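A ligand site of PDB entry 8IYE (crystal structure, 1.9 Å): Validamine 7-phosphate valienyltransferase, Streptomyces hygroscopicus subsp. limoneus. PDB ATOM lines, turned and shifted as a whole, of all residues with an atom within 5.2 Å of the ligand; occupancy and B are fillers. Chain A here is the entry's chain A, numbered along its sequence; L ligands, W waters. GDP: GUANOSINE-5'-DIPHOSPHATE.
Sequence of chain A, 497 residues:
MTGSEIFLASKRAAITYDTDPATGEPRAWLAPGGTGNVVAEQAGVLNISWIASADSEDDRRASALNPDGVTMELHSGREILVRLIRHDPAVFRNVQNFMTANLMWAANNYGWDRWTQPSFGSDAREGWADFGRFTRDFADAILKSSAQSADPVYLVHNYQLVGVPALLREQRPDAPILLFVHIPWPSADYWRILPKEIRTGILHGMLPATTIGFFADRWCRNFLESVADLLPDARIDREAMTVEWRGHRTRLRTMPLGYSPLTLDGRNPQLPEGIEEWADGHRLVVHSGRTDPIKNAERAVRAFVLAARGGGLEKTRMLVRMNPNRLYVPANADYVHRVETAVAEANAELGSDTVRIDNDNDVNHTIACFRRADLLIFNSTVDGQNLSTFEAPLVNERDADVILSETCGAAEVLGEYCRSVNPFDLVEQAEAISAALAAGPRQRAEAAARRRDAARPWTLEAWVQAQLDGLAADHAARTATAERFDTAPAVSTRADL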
ATOM      1  N   SER A 288      11.461  29.117  28.809  1.00  0.00           N
ATOM      2  CA  SER A 288      11.595  28.198  27.687  1.00  0.00           C
ATOM      3  C   SER A 288      11.707  28.984  26.387  1.00  0.00           C
ATOM      4  O   SER A 288      11.000  29.975  26.187  1.00  0.00           O
ATOM      5  CB  SER A 288      10.395  27.242  27.613  1.00  0.00           C
ATOM      6  OG  SER A 288      10.517  26.357  26.511  1.00  0.00           O
ATOM      7  N   ARG A 290      13.951  28.889  22.181  1.00  0.00           N
ATOM      8  CA  ARG A 290      14.999  28.430  21.289  1.00  0.00           C
ATOM      9  C   ARG A 290      16.347  29.028  21.704  1.00  0.00           C
ATOM     10  O   ARG A 290      16.425  30.009  22.435  1.00  0.00           O
ATOM     11  CB  ARG A 290      14.673  28.841  19.852  1.00  0.00           C
ATOM     12  CG  ARG A 290      13.823  27.847  19.095  1.00  0.00           C
ATOM     13  CD  ARG A 290      13.843  28.159  17.610  1.00  0.00           C
ATOM     14  NE  ARG A 290      13.122  29.396  17.353  1.00  0.00           N
ATOM     15  CZ  ARG A 290      13.706  30.565  17.141  1.00  0.00           C
ATOM     16  NH1 ARG A 290      15.019  30.687  17.086  1.00  0.00           N
ATOM     17  NH2 ARG A 290      12.943  31.647  16.998  1.00  0.00           N
ATOM     18  N   ILE A 294      17.071  36.430  21.041  1.00  0.00           N
ATOM     19  CA  ILE A 294      15.852  37.162  21.368  1.00  0.00           C
ATOM     20  C   ILE A 294      15.106  36.560  22.557  1.00  0.00           C
ATOM     21  O   ILE A 294      14.283  37.248  23.171  1.00  0.00           O
ATOM     22  CB  ILE A 294      14.922  37.253  20.138  1.00  0.00           C
ATOM     23  CG1 ILE A 294      14.219  35.917  19.876  1.00  0.00           C
ATOM     24  CG2 ILE A 294      15.690  37.742  18.923  1.00  0.00           C
ATOM     25  CD1 ILE A 294      13.288  35.945  18.687  1.00  0.00           C
ATOM     26  N   LYS A 295      15.370  35.298  22.919  1.00  0.00           N
ATOM     27  CA  LYS A 295      14.589  34.659  23.984  1.00  0.00           C
ATOM     28  C   LYS A 295      14.963  35.157  25.380  1.00  0.00           C
ATOM     29  O   LYS A 295      14.183  34.943  26.317  1.00  0.00           O
ATOM     30  CB  LYS A 295      14.745  33.135  23.902  1.00  0.00           C
ATOM     31  CG  LYS A 295      14.207  32.553  22.605  1.00  0.00           C
ATOM     32  CD  LYS A 295      12.726  32.867  22.419  1.00  0.00           C
ATOM     33  CE  LYS A 295      12.307  32.694  20.970  1.00  0.00           C
ATOM     34  NZ  LYS A 295      10.828  32.820  20.798  1.00  0.00           N
ATOM     35  N   ARG A 321      14.773  25.997  30.145  1.00  0.00           N
ATOM     36  CA  ARG A 321      14.562  25.014  29.089  1.00  0.00           C
ATOM     37  C   ARG A 321      14.907  25.629  27.749  1.00  0.00           C
ATOM     38  O   ARG A 321      14.479  26.749  27.429  1.00  0.00           O
ATOM     39  CB  ARG A 321      13.116  24.512  29.082  1.00  0.00           C
ATOM     40  CG  ARG A 321      12.779  23.663  27.886  1.00  0.00           C
ATOM     41  CD  ARG A 321      12.624  22.206  28.263  1.00  0.00           C
ATOM     42  NE  ARG A 321      12.120  21.411  27.143  1.00  0.00           N
ATOM     43  CZ  ARG A 321      12.785  20.406  26.594  1.00  0.00           C
ATOM     44  NH1 ARG A 321      13.967  20.023  27.037  1.00  0.00           N
ATOM     45  NH2 ARG A 321      12.244  19.755  25.561  1.00  0.00           N
ATOM     46  N   MET A 322      15.687  24.910  26.945  1.00  0.00           N
ATOM     47  CA  MET A 322      16.290  25.517  25.767  1.00  0.00           C
ATOM     48  C   MET A 322      16.124  24.579  24.590  1.00  0.00           C
ATOM     49  O   MET A 322      16.232  23.359  24.726  1.00  0.00           O
ATOM     50  CB  MET A 322      17.760  25.829  26.049  1.00  0.00           C
ATOM     51  CG  MET A 322      18.019  27.305  26.263  1.00  0.00           C
ATOM     52  SD  MET A 322      19.760  27.670  26.563  1.00  0.00           S
ATOM     53  CE  MET A 322      19.803  29.399  26.145  1.00  0.00           C
ATOM     54  N   ASN A 323      15.841  25.167  23.428  1.00  0.00           N
ATOM     55  CA  ASN A 323      15.615  24.400  22.208  1.00  0.00           C
ATOM     56  C   ASN A 323      16.771  24.631  21.247  1.00  0.00           C
ATOM     57  O   ASN A 323      16.909  25.736  20.696  1.00  0.00           O
ATOM     58  CB  ASN A 323      14.279  24.805  21.567  1.00  0.00           C
ATOM     59  CG  ASN A 323      13.974  24.020  20.315  1.00  0.00           C
ATOM     60  OD1 ASN A 323      14.743  23.156  19.914  1.00  0.00           O
ATOM     61  ND2 ASN A 323      12.827  24.304  19.695  1.00  0.00           N
ATOM     62  N   ASP A 360      17.190  20.549  24.580  1.00  0.00           N
ATOM     63  CA  ASP A 360      16.676  19.383  23.858  1.00  0.00           C
ATOM     64  C   ASP A 360      15.523  19.782  22.937  1.00  0.00           C
ATOM     65  O   ASP A 360      14.988  20.892  23.055  1.00  0.00           O
ATOM     66  CB  ASP A 360      16.246  18.286  24.858  1.00  0.00           C
ATOM     67  CG  ASP A 360      15.418  17.186  24.243  1.00  0.00           C
ATOM     68  OD1 ASP A 360      15.696  16.800  23.086  1.00  0.00           O
ATOM     69  OD2 ASP A 360      14.498  16.694  24.927  1.00  0.00           O
ATOM     70  N   ASN A 361      15.203  18.905  21.976  1.00  0.00           N
ATOM     71  CA  ASN A 361      14.085  19.066  21.037  1.00  0.00           C
ATOM     72  C   ASN A 361      12.794  18.324  21.391  1.00  0.00           C
ATOM     73  O   ASN A 361      11.836  18.382  20.612  1.00  0.00           O
ATOM     74  CB  ASN A 361      14.462  18.621  19.620  1.00  0.00           C
ATOM     75  CG  ASN A 361      15.172  19.685  18.848  1.00  0.00           C
ATOM     76  OD1 ASN A 361      15.039  20.847  19.151  1.00  0.00           O
ATOM     77  ND2 ASN A 361      15.879  19.294  17.780  1.00  0.00           N
ATOM     78  N   ASP A 362      12.741  17.612  22.511  1.00  0.00           N
ATOM     79  CA  ASP A 362      11.512  16.898  22.836  1.00  0.00           C
ATOM     80  C   ASP A 362      10.445  17.911  23.195  1.00  0.00           C
ATOM     81  O   ASP A 362      10.469  18.505  24.287  1.00  0.00           O
ATOM     82  CB  ASP A 362      11.744  15.898  23.963  1.00  0.00           C
ATOM     83  CG  ASP A 362      10.592  14.934  24.136  1.00  0.00           C
ATOM     84  OD1 ASP A 362       9.620  14.988  23.356  1.00  0.00           O
ATOM     85  OD2 ASP A 362      10.660  14.130  25.085  1.00  0.00           O
ATOM     86  N   VAL A 363       9.499  18.103  22.282  1.00  0.00           N
ATOM     87  CA  VAL A 363       8.427  19.067  22.484  1.00  0.00           C
ATOM     88  C   VAL A 363       7.546  18.610  23.634  1.00  0.00           C
ATOM     89  O   VAL A 363       6.969  19.428  24.354  1.00  0.00           O
ATOM     90  CB  VAL A 363       7.653  19.246  21.153  1.00  0.00           C
ATOM     91  CG1 VAL A 363       6.926  17.963  20.775  1.00  0.00           C
ATOM     92  CG2 VAL A 363       6.701  20.441  21.203  1.00  0.00           C
ATOM     93  N   THR A 366       8.965  19.870  26.866  1.00  0.00           N
ATOM     94  CA  THR A 366       8.669  21.275  27.125  1.00  0.00           C
ATOM     95  C   THR A 366       7.245  21.445  27.645  1.00  0.00           C
ATOM     96  O   THR A 366       7.018  22.222  28.587  1.00  0.00           O
ATOM     97  CB  THR A 366       8.884  22.099  25.856  1.00  0.00           C
ATOM     98  OG1 THR A 366      10.263  22.051  25.472  1.00  0.00           O
ATOM     99  CG2 THR A 366       8.479  23.552  26.089  1.00  0.00           C
ATOM    100  N   ILE A 367       6.284  20.736  27.055  1.00  0.00           N
ATOM    101  CA  ILE A 367       4.917  20.773  27.551  1.00  0.00           C
ATOM    102  C   ILE A 367       4.866  20.258  28.984  1.00  0.00           C
ATOM    103  O   ILE A 367       4.131  20.782  29.836  1.00  0.00           O
ATOM    104  CB  ILE A 367       3.986  19.965  26.635  1.00  0.00           C
ATOM    105  CG1 ILE A 367       4.106  20.434  25.176  1.00  0.00           C
ATOM    106  CG2 ILE A 367       2.544  20.066  27.107  1.00  0.00           C
ATOM    107  CD1 ILE A 367       4.071  21.948  25.010  1.00  0.00           C
ATOM    108  N   PHE A 370       5.945  23.011  31.035  1.00  0.00           N
ATOM    109  CA  PHE A 370       4.856  23.967  31.140  1.00  0.00           C
ATOM    110  C   PHE A 370       3.884  23.581  32.250  1.00  0.00           C
ATOM    111  O   PHE A 370       3.451  24.441  33.029  1.00  0.00           O
ATOM    112  CB  PHE A 370       4.111  24.072  29.816  1.00  0.00           C
ATOM    113  CG  PHE A 370       4.852  24.841  28.756  1.00  0.00           C
ATOM    114  CD1 PHE A 370       5.925  25.657  29.070  1.00  0.00           C
ATOM    115  CD2 PHE A 370       4.457  24.768  27.419  1.00  0.00           C
ATOM    116  CE1 PHE A 370       6.602  26.361  28.091  1.00  0.00           C
ATOM    117  CE2 PHE A 370       5.121  25.468  26.439  1.00  0.00           C
ATOM    118  CZ  PHE A 370       6.201  26.273  26.779  1.00  0.00           C
ATOM    119  N   ASP A 383       9.735  39.536  19.895  1.00  0.00           N
ATOM    120  CA  ASP A 383       9.251  38.269  19.369  1.00  0.00           C
ATOM    121  C   ASP A 383       8.091  38.548  18.419  1.00  0.00           C
ATOM    122  O   ASP A 383       7.170  39.294  18.771  1.00  0.00           O
ATOM    123  CB  ASP A 383       8.802  37.336  20.497  1.00  0.00           C
ATOM    124  CG  ASP A 383       9.405  35.947  20.369  1.00  0.00           C
ATOM    125  OD1 ASP A 383       9.410  35.390  19.251  1.00  0.00           O
ATOM    126  OD2 ASP A 383       9.878  35.423  21.402  1.00  0.00           O
ATOM    127  N   GLN A 385       5.596  36.771  17.656  1.00  0.00           N
ATOM    128  CA  GLN A 385       4.404  36.531  18.443  1.00  0.00           C
ATOM    129  C   GLN A 385       4.725  35.831  19.764  1.00  0.00           C
ATOM    130  O   GLN A 385       4.341  36.311  20.828  1.00  0.00           O
ATOM    131  CB  GLN A 385       3.390  35.700  17.655  1.00  0.00           C
ATOM    132  CG  GLN A 385       2.104  35.432  18.431  1.00  0.00           C
ATOM    133  CD  GLN A 385       1.175  36.641  18.502  1.00  0.00           C
ATOM    134  OE1 GLN A 385       1.572  37.775  18.262  1.00  0.00           O
ATOM    135  NE2 GLN A 385      -0.071  36.377  18.848  1.00  0.00           N
ATOM    136  N   ASN A 386       5.426  34.697  19.675  1.00  0.00           N
ATOM    137  CA  ASN A 386       5.715  33.788  20.776  1.00  0.00           C
ATOM    138  C   ASN A 386       4.452  33.004  21.127  1.00  0.00           C
ATOM    139  O   ASN A 386       3.609  33.472  21.898  1.00  0.00           O
ATOM    140  CB  ASN A 386       6.289  34.533  21.989  1.00  0.00           C
ATOM    141  CG  ASN A 386       6.729  33.609  23.114  1.00  0.00           C
ATOM    142  OD1 ASN A 386       6.050  32.637  23.450  1.00  0.00           O
ATOM    143  ND2 ASN A 386       7.884  33.892  23.692  1.00  0.00           N
ATOM    144  N   LEU A 387       4.324  31.809  20.546  1.00  0.00           N
ATOM    145  CA  LEU A 387       3.186  30.935  20.811  1.00  0.00           C
ATOM    146  C   LEU A 387       3.290  30.230  22.164  1.00  0.00           C
ATOM    147  O   LEU A 387       2.260  29.796  22.680  1.00  0.00           O
ATOM    148  CB  LEU A 387       3.053  29.885  19.707  1.00  0.00           C
ATOM    149  CG  LEU A 387       3.063  30.349  18.248  1.00  0.00           C
ATOM    150  CD1 LEU A 387       2.542  29.235  17.328  1.00  0.00           C
ATOM    151  CD2 LEU A 387       2.238  31.605  18.072  1.00  0.00           C
ATOM    152  N   SER A 388       4.492  30.088  22.709  1.00  0.00           N
ATOM    153  CA  SER A 388       4.648  29.410  23.989  1.00  0.00           C
ATOM    154  C   SER A 388       3.887  30.115  25.110  1.00  0.00           C
ATOM    155  O   SER A 388       3.389  29.457  26.027  1.00  0.00           O
ATOM    156  CB  SER A 388       6.133  29.290  24.351  1.00  0.00           C
ATOM    157  OG  SER A 388       6.804  28.421  23.464  1.00  0.00           O
ATOM    158  N   GLU A 391       0.480  28.597  24.838  1.00  0.00           N
ATOM    159  CA  GLU A 391       0.417  27.171  25.171  1.00  0.00           C
ATOM    160  C   GLU A 391       0.608  26.946  26.663  1.00  0.00           C
ATOM    161  O   GLU A 391      -0.112  26.131  27.273  1.00  0.00           O
ATOM    162  CB  GLU A 391       1.503  26.406  24.412  1.00  0.00           C
ATOM    163  CG  GLU A 391       1.255  26.187  22.947  1.00  0.00           C
ATOM    164  CD  GLU A 391       2.535  25.775  22.238  1.00  0.00           C
ATOM    165  OE1 GLU A 391       3.555  25.568  22.925  1.00  0.00           O
ATOM    166  OE2 GLU A 391       2.522  25.654  20.994  1.00  0.00           O
HETATM  167  PB  GDP L   1       9.725  30.677  17.983  1.00  0.00           P
HETATM  168  O1B GDP L   1       8.709  30.028  17.077  1.00  0.00           O
HETATM  169  O2B GDP L   1      10.895  29.790  18.342  1.00  0.00           O
HETATM  170  O3B GDP L   1      10.140  32.075  17.560  1.00  0.00           O
HETATM  171  O3A GDP L   1       8.990  30.901  19.404  1.00  0.00           O
HETATM  172  PA  GDP L   1       7.466  30.458  19.726  1.00  0.00           P
HETATM  173  O1A GDP L   1       6.526  31.229  18.831  1.00  0.00           O
HETATM  174  O2A GDP L   1       7.272  30.477  21.224  1.00  0.00           O
HETATM  175  O5' GDP L   1       7.450  28.927  19.227  1.00  0.00           O
HETATM  176  C5' GDP L   1       7.817  27.886  20.118  1.00  0.00           C
HETATM  177  C4' GDP L   1       7.124  26.609  19.691  1.00  0.00           C
HETATM  178  O4' GDP L   1       8.058  25.537  19.739  1.00  0.00           O
HETATM  179  C3' GDP L   1       5.990  26.281  20.644  1.00  0.00           C
HETATM  180  O3' GDP L   1       4.875  25.810  19.876  1.00  0.00           O
HETATM  181  C2' GDP L   1       6.511  25.139  21.490  1.00  0.00           C
HETATM  182  O2' GDP L   1       5.492  24.209  21.838  1.00  0.00           O
HETATM  183  C1' GDP L   1       7.535  24.500  20.562  1.00  0.00           C
HETATM  184  N9  GDP L   1       8.618  23.870  21.337  1.00  0.00           N
HETATM  185  C8  GDP L   1       8.925  24.105  22.628  1.00  0.00           C
HETATM  186  N7  GDP L   1       9.977  23.353  23.018  1.00  0.00           N
HETATM  187  C5  GDP L   1      10.363  22.613  21.958  1.00  0.00           C
HETATM  188  C6  GDP L   1      11.411  21.614  21.677  1.00  0.00           C
HETATM  189  O6  GDP L   1      12.220  21.264  22.566  1.00  0.00           O
HETATM  190  N1  GDP L   1      11.464  21.089  20.441  1.00  0.00           N
HETATM  191  C2  GDP L   1      10.605  21.443  19.466  1.00  0.00           C
HETATM  192  N2  GDP L   1      10.729  20.877  18.236  1.00  0.00           N
HETATM  193  N3  GDP L   1       9.621  22.364  19.656  1.00  0.00           N
HETATM  194  C4  GDP L   1       9.463  22.955  20.850  1.00  0.00           C
HETATM  195  O   HOH W   1       9.502  30.840  22.498  1.00  0.00           O
HETATM  196  O   HOH W   2      10.938  32.262  14.165  1.00  0.00           O
HETATM  197  O   HOH W   3      11.526  29.507  20.985  1.00  0.00           O
HETATM  198  O   HOH W   4       6.110  33.404  17.258  1.00  0.00           O
HETATM  199  O   HOH W   5       9.701  30.156  14.399  1.00  0.00           O
HETATM  200  O   HOH W   6       8.979  27.134  24.236  1.00  0.00           O
HETATM  201  O   HOH W   7      13.596  22.738  24.213  1.00  0.00           O
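The backbone carbonyl oxygen of Asp 360 lies close to an oxygen (O6) of the ligand (2.8 Å).
Asn 323 touches the ligand.
Asp 362 touches the ligand.
Val 363 touches the ligand.
OD1 of Asp 383 touches O3B of the ligand, 3.8 Å away.
Hydrophobic or aromatic side chains that line the ligand: Val 363 and Leu 387.
14 residues have an atom within 4 Å of the ligand: Arg 290, Lys 295, Arg 321, Asn 323, Asp 360, Asn 361, Asp 362, Val 363, Thr 366, Asp 383, Asn 386, Leu 387, Ser 388 and Glu 391.
The nearest printed residue that does not touch the ligand is Ile 367 (4.1 Å).
Water W1 lies within hydrogen-bond range of an oxygen (O2A) of the ligand and the side-chain amino group (NZ) of Lys 295.
Water W4 lies within hydrogen-bond range of an oxygen (O1A) of the ligand, the backbone NH of Asn 386 and the backbone NH of Gln 385.
Water W3 lies within hydrogen-bond range of O2B of the ligand, N of Arg 290 and NZ of Lys 295.
Water W6 lies within hydrogen-bond range of OG of Ser 388 (2.6 Å) and OG of Ser 288 (2.9 Å).
The side-chain amide oxygen (OD1) of Asn 361 lies close to the side-chain amide oxygen (OD1) of Asn 323 (2.4 Å).
The guanidinium group of Arg 321 sits at hydrogen-bond distance from the side-chain hydroxyl of Thr 366.
The side-chain carboxylate (OD1) of Asp 360 is in hydrogen-bond range of the backbone NH (N) of Asp 362.
N of Asp 360 lies within hydrogen-bond range of O of Met 322, 3.0 Å away.
NZ of Lys 295 is in salt-bridge range of OD2 of Asp 383, at 2.8 Å.
The side-chain amide oxygen (OD1) of Asn 386 lies within hydrogen-bond range of the backbone NH (N) of Ser 388 (3.1 Å).
The side-chain amide nitrogen (ND2) of Asn 386 is in hydrogen-bond range of the side-chain carboxylate (OD2) of Asp 383.
The backbone carbonyl oxygen (O) of Asp 362 sits at hydrogen-bond distance from the guanidinium group (NH2) of Arg 321 (2.5 Å).
NE of Arg 290 is in salt-bridge range of O2B of the ligand (2.5 Å).
The side-chain carboxylate of Glu 391 lies within hydrogen-bond range of an oxygen (O2') of the ligand (2.6 Å).
A nitrogen (N1) of the ligand sits at hydrogen-bond distance from the backbone carbonyl oxygen (O) of Asn 361.
N7 of the ligand lies within hydrogen-bond range of OG1 of Thr 366 (2.8 Å).
An oxygen (O1A) of the ligand sits at hydrogen-bond distance from the backbone NH (N) of Leu 387 (2.9 Å).
NZ of Lys 295 lies within salt-bridge range of O3B of the ligand (3.4 Å).
N of Ser 388 is in hydrogen-bond range of O2A of the ligand.
O2A of the ligand is in hydrogen-bond range of OG of Ser 388 (3.1 Å).
An oxygen (O2A) of the ligand lies close to the side-chain amide oxygen of Asn 386.
NH2 of Arg 321 lies within hydrogen-bond range of O6 of the ligand (3.4 Å).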
